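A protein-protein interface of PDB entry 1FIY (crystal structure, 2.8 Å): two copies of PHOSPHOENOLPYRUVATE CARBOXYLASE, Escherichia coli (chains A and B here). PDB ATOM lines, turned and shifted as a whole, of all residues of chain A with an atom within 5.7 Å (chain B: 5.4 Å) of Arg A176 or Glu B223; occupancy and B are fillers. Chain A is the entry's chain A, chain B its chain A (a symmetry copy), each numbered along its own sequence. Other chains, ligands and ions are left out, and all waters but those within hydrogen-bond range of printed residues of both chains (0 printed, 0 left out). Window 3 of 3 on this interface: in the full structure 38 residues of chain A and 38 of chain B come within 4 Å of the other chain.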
ATOM      1  N   HIS A 171     -15.161  11.859  -2.652  1.00  0.00           N
ATOM      2  CA  HIS A 171     -14.834  11.568  -4.039  1.00  0.00           C
ATOM      3  C   HIS A 171     -13.409  11.071  -4.183  1.00  0.00           C
ATOM      4  O   HIS A 171     -13.116  10.127  -4.909  1.00  0.00           O
ATOM      5  CB  HIS A 171     -15.051  12.820  -4.888  1.00  0.00           C
ATOM      6  CG  HIS A 171     -14.955  12.569  -6.359  1.00  0.00           C
ATOM      7  ND1 HIS A 171     -13.752  12.581  -7.031  1.00  0.00           N
ATOM      8  CD2 HIS A 171     -15.914  12.300  -7.280  1.00  0.00           C
ATOM      9  CE1 HIS A 171     -13.964  12.334  -8.307  1.00  0.00           C
ATOM     10  NE2 HIS A 171     -15.263  12.153  -8.483  1.00  0.00           N
ATOM     11  N   ASN A 172     -12.491  11.708  -3.475  1.00  0.00           N
ATOM     12  CA  ASN A 172     -11.077  11.376  -3.470  1.00  0.00           C
ATOM     13  C   ASN A 172     -10.878   9.962  -2.925  1.00  0.00           C
ATOM     14  O   ASN A 172     -10.087   9.171  -3.439  1.00  0.00           O
ATOM     15  CB  ASN A 172     -10.325  12.418  -2.637  1.00  0.00           C
ATOM     16  CG  ASN A 172      -8.816  12.322  -2.717  1.00  0.00           C
ATOM     17  OD1 ASN A 172      -8.160  11.505  -2.056  1.00  0.00           O
ATOM     18  ND2 ASN A 172      -8.212  13.180  -3.544  1.00  0.00           N
ATOM     19  N   GLN A 173     -11.621   9.653  -1.863  1.00  0.00           N
ATOM     20  CA  GLN A 173     -11.563   8.341  -1.227  1.00  0.00           C
ATOM     21  C   GLN A 173     -12.053   7.269  -2.204  1.00  0.00           C
ATOM     22  O   GLN A 173     -11.409   6.242  -2.440  1.00  0.00           O
ATOM     23  CB  GLN A 173     -12.389   8.364   0.061  1.00  0.00           C
ATOM     24  CG  GLN A 173     -11.740   9.035   1.241  1.00  0.00           C
ATOM     25  CD  GLN A 173     -12.664   9.443   2.365  1.00  0.00           C
ATOM     26  OE1 GLN A 173     -13.756   8.906   2.585  1.00  0.00           O
ATOM     27  NE2 GLN A 173     -12.256  10.444   3.157  1.00  0.00           N
ATOM     28  N   LEU A 174     -13.221   7.555  -2.805  1.00  0.00           N
ATOM     29  CA  LEU A 174     -13.826   6.649  -3.782  1.00  0.00           C
ATOM     30  C   LEU A 174     -12.877   6.398  -4.937  1.00  0.00           C
ATOM     31  O   LEU A 174     -12.506   5.268  -5.270  1.00  0.00           O
ATOM     32  CB  LEU A 174     -15.169   7.202  -4.234  1.00  0.00           C
ATOM     33  CG  LEU A 174     -16.313   7.055  -3.224  1.00  0.00           C
ATOM     34  CD1 LEU A 174     -17.583   7.717  -3.719  1.00  0.00           C
ATOM     35  CD2 LEU A 174     -16.561   5.593  -2.906  1.00  0.00           C
ATOM     36  N   MET A 175     -12.368   7.465  -5.547  1.00  0.00           N
ATOM     37  CA  MET A 175     -11.399   7.279  -6.628  1.00  0.00           C
ATOM     38  C   MET A 175     -10.180   6.488  -6.181  1.00  0.00           C
ATOM     39  O   MET A 175      -9.587   5.748  -6.985  1.00  0.00           O
ATOM     40  CB  MET A 175     -11.045   8.648  -7.213  1.00  0.00           C
ATOM     41  CG  MET A 175     -12.084   9.220  -8.143  1.00  0.00           C
ATOM     42  SD  MET A 175     -12.542   8.141  -9.518  1.00  0.00           S
ATOM     43  CE  MET A 175     -11.126   8.362 -10.592  1.00  0.00           C
ATOM     44  N   ARG A 176      -9.732   6.602  -4.939  1.00  0.00           N
ATOM     45  CA  ARG A 176      -8.568   5.902  -4.406  1.00  0.00           C
ATOM     46  C   ARG A 176      -8.766   4.387  -4.417  1.00  0.00           C
ATOM     47  O   ARG A 176      -7.869   3.636  -4.784  1.00  0.00           O
ATOM     48  CB  ARG A 176      -8.252   6.391  -2.991  1.00  0.00           C
ATOM     49  CG  ARG A 176      -6.876   6.045  -2.450  1.00  0.00           C
ATOM     50  CD  ARG A 176      -6.569   6.782  -1.144  1.00  0.00           C
ATOM     51  NE  ARG A 176      -7.574   6.534  -0.113  1.00  0.00           N
ATOM     52  CZ  ARG A 176      -8.136   7.476   0.637  1.00  0.00           C
ATOM     53  NH1 ARG A 176      -7.792   8.750   0.493  1.00  0.00           N
ATOM     54  NH2 ARG A 176      -9.052   7.169   1.550  1.00  0.00           N
ATOM     55  N   ARG A 177      -9.956   3.937  -4.036  1.00  0.00           N
ATOM     56  CA  ARG A 177     -10.287   2.522  -4.064  1.00  0.00           C
ATOM     57  C   ARG A 177     -10.424   2.044  -5.511  1.00  0.00           C
ATOM     58  O   ARG A 177      -9.903   0.997  -5.894  1.00  0.00           O
ATOM     59  CB  ARG A 177     -11.596   2.239  -3.331  1.00  0.00           C
ATOM     60  CG  ARG A 177     -11.900   0.765  -3.177  1.00  0.00           C
ATOM     61  CD  ARG A 177     -10.759  -0.020  -2.547  1.00  0.00           C
ATOM     62  NE  ARG A 177     -11.250  -1.276  -1.994  1.00  0.00           N
ATOM     63  CZ  ARG A 177     -10.632  -2.445  -2.020  1.00  0.00           C
ATOM     64  NH1 ARG A 177      -9.434  -2.613  -2.575  1.00  0.00           N
ATOM     65  NH2 ARG A 177     -11.221  -3.501  -1.463  1.00  0.00           N
ATOM     66  N   LEU A 178     -11.109   2.844  -6.326  1.00  0.00           N
ATOM     67  CA  LEU A 178     -11.308   2.557  -7.735  1.00  0.00           C
ATOM     68  C   LEU A 178      -9.977   2.294  -8.418  1.00  0.00           C
ATOM     69  O   LEU A 178      -9.829   1.315  -9.141  1.00  0.00           O
ATOM     70  CB  LEU A 178     -12.039   3.684  -8.443  1.00  0.00           C
ATOM     71  CG  LEU A 178     -12.455   3.401  -9.887  1.00  0.00           C
ATOM     72  CD1 LEU A 178     -13.539   2.335  -9.914  1.00  0.00           C
ATOM     73  CD2 LEU A 178     -12.931   4.681 -10.560  1.00  0.00           C
ATOM     74  N   ARG A 179      -9.009   3.156  -8.148  1.00  0.00           N
ATOM     75  CA  ARG A 179      -7.659   3.006  -8.695  1.00  0.00           C
ATOM     76  C   ARG A 179      -7.026   1.694  -8.234  1.00  0.00           C
ATOM     77  O   ARG A 179      -6.412   0.938  -8.990  1.00  0.00           O
ATOM     78  CB  ARG A 179      -6.858   4.234  -8.267  1.00  0.00           C
ATOM     79  CG  ARG A 179      -5.548   4.425  -9.004  1.00  0.00           C
ATOM     80  CD  ARG A 179      -5.297   5.917  -9.278  1.00  0.00           C
ATOM     81  NE  ARG A 179      -4.158   6.021 -10.217  1.00  0.00           N
ATOM     82  CZ  ARG A 179      -2.900   5.965  -9.769  1.00  0.00           C
ATOM     83  NH1 ARG A 179      -2.675   5.829  -8.463  1.00  0.00           N
ATOM     84  NH2 ARG A 179      -1.891   6.049 -10.638  1.00  0.00           N
ATOM     85  N   GLN A 180      -7.211   1.403  -6.944  1.00  0.00           N
ATOM     86  CA  GLN A 180      -6.719   0.193  -6.314  1.00  0.00           C
ATOM     87  C   GLN A 180      -7.259  -1.030  -7.056  1.00  0.00           C
ATOM     88  O   GLN A 180      -6.501  -1.886  -7.536  1.00  0.00           O
ATOM     89  CB  GLN A 180      -7.093   0.197  -4.834  1.00  0.00           C
ATOM     90  CG  GLN A 180      -5.950  -0.019  -3.864  1.00  0.00           C
ATOM     91  CD  GLN A 180      -5.981   0.848  -2.613  1.00  0.00           C
ATOM     92  OE1 GLN A 180      -6.929   0.821  -1.816  1.00  0.00           O
ATOM     93  NE2 GLN A 180      -4.910   1.637  -2.422  1.00  0.00           N
ATOM     94  N   LEU A 181      -8.581  -1.103  -7.166  1.00  0.00           N
ATOM     95  CA  LEU A 181      -9.325  -2.145  -7.857  1.00  0.00           C
ATOM     96  C   LEU A 181      -8.898  -2.292  -9.311  1.00  0.00           C
ATOM     97  O   LEU A 181      -8.740  -3.405  -9.822  1.00  0.00           O
ATOM     98  CB  LEU A 181     -10.806  -1.792  -7.811  1.00  0.00           C
ATOM     99  CG  LEU A 181     -11.809  -2.586  -7.004  1.00  0.00           C
ATOM    100  CD1 LEU A 181     -11.211  -3.811  -6.345  1.00  0.00           C
ATOM    101  CD2 LEU A 181     -12.534  -1.724  -5.982  1.00  0.00           C
ATOM    102  N   PRO B 101     -10.839  16.078   5.932  1.00  0.00           N
ATOM    103  CA  PRO B 101      -9.417  16.280   6.043  1.00  0.00           C
ATOM    104  C   PRO B 101      -8.900  17.687   6.186  1.00  0.00           C
ATOM    105  O   PRO B 101      -7.680  17.834   6.439  1.00  0.00           O
ATOM    106  CB  PRO B 101      -8.865  15.624   4.779  1.00  0.00           C
ATOM    107  CG  PRO B 101      -9.871  14.593   4.420  1.00  0.00           C
ATOM    108  CD  PRO B 101     -11.204  15.172   4.814  1.00  0.00           C
ATOM    109  N   PRO B 218      -6.295   3.065  10.135  1.00  0.00           N
ATOM    110  CA  PRO B 218      -5.667   3.157   8.820  1.00  0.00           C
ATOM    111  C   PRO B 218      -6.202   4.292   7.960  1.00  0.00           C
ATOM    112  O   PRO B 218      -5.423   4.936   7.232  1.00  0.00           O
ATOM    113  CB  PRO B 218      -5.855   1.783   8.198  1.00  0.00           C
ATOM    114  CG  PRO B 218      -6.185   0.878   9.330  1.00  0.00           C
ATOM    115  CD  PRO B 218      -6.892   1.727  10.373  1.00  0.00           C
ATOM    116  N   ASN B 219      -7.502   4.591   8.005  1.00  0.00           N
ATOM    117  CA  ASN B 219      -8.073   5.696   7.247  1.00  0.00           C
ATOM    118  C   ASN B 219      -7.489   7.000   7.797  1.00  0.00           C
ATOM    119  O   ASN B 219      -7.022   7.875   7.068  1.00  0.00           O
ATOM    120  CB  ASN B 219      -9.586   5.736   7.341  1.00  0.00           C
ATOM    121  CG  ASN B 219     -10.267   4.560   6.661  1.00  0.00           C
ATOM    122  OD1 ASN B 219      -9.662   3.937   5.797  1.00  0.00           O
ATOM    123  ND2 ASN B 219     -11.486   4.256   7.062  1.00  0.00           N
ATOM    124  N   TYR B 220      -7.457   7.093   9.132  1.00  0.00           N
ATOM    125  CA  TYR B 220      -6.831   8.241   9.779  1.00  0.00           C
ATOM    126  C   TYR B 220      -5.395   8.357   9.258  1.00  0.00           C
ATOM    127  O   TYR B 220      -4.974   9.437   8.837  1.00  0.00           O
ATOM    128  CB  TYR B 220      -6.840   8.162  11.291  1.00  0.00           C
ATOM    129  CG  TYR B 220      -5.654   8.841  11.937  1.00  0.00           C
ATOM    130  CD1 TYR B 220      -5.451  10.206  11.794  1.00  0.00           C
ATOM    131  CD2 TYR B 220      -4.727   8.124  12.674  1.00  0.00           C
ATOM    132  CE1 TYR B 220      -4.361  10.832  12.367  1.00  0.00           C
ATOM    133  CE2 TYR B 220      -3.641   8.740  13.257  1.00  0.00           C
ATOM    134  CZ  TYR B 220      -3.456  10.096  13.097  1.00  0.00           C
ATOM    135  OH  TYR B 220      -2.376  10.720  13.669  1.00  0.00           O
ATOM    136  N   LEU B 221      -4.643   7.279   9.237  1.00  0.00           N
ATOM    137  CA  LEU B 221      -3.272   7.303   8.746  1.00  0.00           C
ATOM    138  C   LEU B 221      -3.158   7.621   7.271  1.00  0.00           C
ATOM    139  O   LEU B 221      -2.141   8.205   6.842  1.00  0.00           O
ATOM    140  CB  LEU B 221      -2.576   5.986   9.117  1.00  0.00           C
ATOM    141  CG  LEU B 221      -2.109   5.937  10.586  1.00  0.00           C
ATOM    142  CD1 LEU B 221      -2.356   4.560  11.181  1.00  0.00           C
ATOM    143  CD2 LEU B 221      -0.639   6.298  10.681  1.00  0.00           C
ATOM    144  N   ARG B 222      -4.164   7.283   6.463  1.00  0.00           N
ATOM    145  CA  ARG B 222      -4.112   7.600   5.032  1.00  0.00           C
ATOM    146  C   ARG B 222      -4.349   9.101   4.845  1.00  0.00           C
ATOM    147  O   ARG B 222      -3.576   9.825   4.211  1.00  0.00           O
ATOM    148  CB  ARG B 222      -5.153   6.787   4.290  1.00  0.00           C
ATOM    149  CG  ARG B 222      -4.614   6.002   3.097  1.00  0.00           C
ATOM    150  CD  ARG B 222      -5.646   5.007   2.622  1.00  0.00           C
ATOM    151  NE  ARG B 222      -5.301   3.591   2.675  1.00  0.00           N
ATOM    152  CZ  ARG B 222      -4.349   3.036   1.940  1.00  0.00           C
ATOM    153  NH1 ARG B 222      -3.628   3.792   1.124  1.00  0.00           N
ATOM    154  NH2 ARG B 222      -4.068   1.755   1.979  1.00  0.00           N
ATOM    155  N   GLU B 223      -5.440   9.590   5.438  1.00  0.00           N
ATOM    156  CA  GLU B 223      -5.748  11.009   5.337  1.00  0.00           C
ATOM    157  C   GLU B 223      -4.578  11.834   5.832  1.00  0.00           C
ATOM    158  O   GLU B 223      -4.049  12.698   5.123  1.00  0.00           O
ATOM    159  CB  GLU B 223      -7.048  11.307   6.059  1.00  0.00           C
ATOM    160  CG  GLU B 223      -8.331  10.804   5.385  1.00  0.00           C
ATOM    161  CD  GLU B 223      -8.272  10.843   3.872  1.00  0.00           C
ATOM    162  OE1 GLU B 223      -7.961  11.923   3.326  1.00  0.00           O
ATOM    163  OE2 GLU B 223      -8.501   9.815   3.208  1.00  0.00           O
ATOM    164  N   LEU B 224      -4.083  11.562   7.047  1.00  0.00           N
ATOM    165  CA  LEU B 224      -2.951  12.264   7.628  1.00  0.00           C
ATOM    166  C   LEU B 224      -1.759  12.306   6.676  1.00  0.00           C
ATOM    167  O   LEU B 224      -1.039  13.297   6.576  1.00  0.00           O
ATOM    168  CB  LEU B 224      -2.475  11.581   8.920  1.00  0.00           C
ATOM    169  CG  LEU B 224      -1.198  12.179   9.533  1.00  0.00           C
ATOM    170  CD1 LEU B 224      -1.557  13.428  10.330  1.00  0.00           C
ATOM    171  CD2 LEU B 224      -0.467  11.172  10.390  1.00  0.00           C
ATOM    172  N   ASN B 225      -1.529  11.182   6.001  1.00  0.00           N
ATOM    173  CA  ASN B 225      -0.428  11.097   5.071  1.00  0.00           C
ATOM    174  C   ASN B 225      -0.674  11.876   3.803  1.00  0.00           C
ATOM    175  O   ASN B 225       0.273  12.456   3.289  1.00  0.00           O
ATOM    176  CB  ASN B 225      -0.100   9.634   4.750  1.00  0.00           C
ATOM    177  CG  ASN B 225       1.283   9.358   5.329  1.00  0.00           C
ATOM    178  OD1 ASN B 225       1.401   9.394   6.547  1.00  0.00           O
ATOM    179  ND2 ASN B 225       2.215   9.135   4.432  1.00  0.00           N
ATOM    180  N   GLU B 226      -1.909  11.896   3.305  1.00  0.00           N
ATOM    181  CA  GLU B 226      -2.182  12.674   2.098  1.00  0.00           C
ATOM    182  C   GLU B 226      -1.924  14.146   2.417  1.00  0.00           C
ATOM    183  O   GLU B 226      -1.268  14.847   1.664  1.00  0.00           O
ATOM    184  CB  GLU B 226      -3.603  12.488   1.610  1.00  0.00           C
ATOM    185  CG  GLU B 226      -3.723  11.999   0.170  1.00  0.00           C
ATOM    186  CD  GLU B 226      -4.127  10.532   0.149  1.00  0.00           C
ATOM    187  OE1 GLU B 226      -5.324  10.260   0.385  1.00  0.00           O
ATOM    188  OE2 GLU B 226      -3.245   9.670  -0.084  1.00  0.00           O
ATOM    189  N   GLN B 227      -2.413  14.610   3.550  1.00  0.00           N
ATOM    190  CA  GLN B 227      -2.238  15.981   3.984  1.00  0.00           C
ATOM    191  C   GLN B 227      -0.810  16.423   4.183  1.00  0.00           C
ATOM    192  O   GLN B 227      -0.463  17.582   3.905  1.00  0.00           O
ATOM    193  CB  GLN B 227      -3.050  16.141   5.287  1.00  0.00           C
ATOM    194  CG  GLN B 227      -4.514  15.765   4.982  1.00  0.00           C
ATOM    195  CD  GLN B 227      -5.154  16.964   4.293  1.00  0.00           C
ATOM    196  OE1 GLN B 227      -5.336  17.939   5.021  1.00  0.00           O
ATOM    197  NE2 GLN B 227      -5.459  16.922   3.017  1.00  0.00           N
ATOM    198  N   LEU B 228       0.067  15.548   4.685  1.00  0.00           N
ATOM    199  CA  LEU B 228       1.462  15.942   4.878  1.00  0.00           C
ATOM    200  C   LEU B 228       2.085  16.227   3.520  1.00  0.00           C
ATOM    201  O   LEU B 228       2.714  17.260   3.322  1.00  0.00           O
ATOM    202  CB  LEU B 228       2.241  14.897   5.640  1.00  0.00           C
ATOM    203  CG  LEU B 228       1.801  14.587   7.069  1.00  0.00           C
ATOM    204  CD1 LEU B 228       2.716  13.521   7.672  1.00  0.00           C
ATOM    205  CD2 LEU B 228       1.765  15.831   7.943  1.00  0.00           C
ATOM    206  N   VAL B 628     -11.736   8.765  12.806  1.00  0.00           N
ATOM    207  CA  VAL B 628     -10.856   9.627  12.017  1.00  0.00           C
ATOM    208  C   VAL B 628     -10.855  11.060  12.527  1.00  0.00           C
ATOM    209  O   VAL B 628      -9.813  11.723  12.665  1.00  0.00           O
ATOM    210  CB  VAL B 628     -11.254   9.543  10.537  1.00  0.00           C
ATOM    211  CG1 VAL B 628     -10.565  10.565   9.668  1.00  0.00           C
ATOM    212  CG2 VAL B 628     -10.924   8.128  10.050  1.00  0.00           C
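The guanidinium group (NH1) of Arg A176 is in salt-bridge range of the side-chain carboxylate (OE2) of Glu B223 (3.0 Å). NH1 of Arg A176 is in salt-bridge range of OE1 of Glu B226, at 2.9 Å.
OD1 of Asn A172 touches OE1 of Glu B226, 3.9 Å away. OE2 of Glu B223 touches NE2 of Gln A173, 3.8 Å away. Arg B222 touches Arg A176 (CD to NE, 3.7 Å).
Printed residues of chain A that touch a printed residue of chain B: Asn A172, Gln A173 and Arg A176. Among the printed residues, 5 pairs touch across the chains.
No position is printed for both chains. Of the 5 pairs that touch across the chains among the printed residues, none has its exchanged pair printed and touching as well.
Of chain B, only Arg B222, Glu B223 and Glu B226 come within 4 Å of Arg A176. Of chain A, only Gln A173 (3.8 Å) and Arg A176 (3.0 Å) come within 4 Å of Glu B223. Printed residues of chain A within 4 Å of Arg B222: Arg A176 (3.7 Å). Of the printed residues of chain B, Asn A172 touches Glu B226 (3.9 Å). Of the printed residues of chain A, Glu B226 touches Asn A172 and Arg A176. Tyr B220 touches none of the printed residues of chain A. Arg A177 touches none of the printed residues of chain B. The nearest printed residue of chain B that does not touch Arg A176 is Asn B219 (5.4 Å). The nearest residue of chain A that does not touch Glu B223 is Asn A172 (5.4 Å). The nearest printed residue of chain A that does not touch Arg B222 is Gln A180 (4.3 Å).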
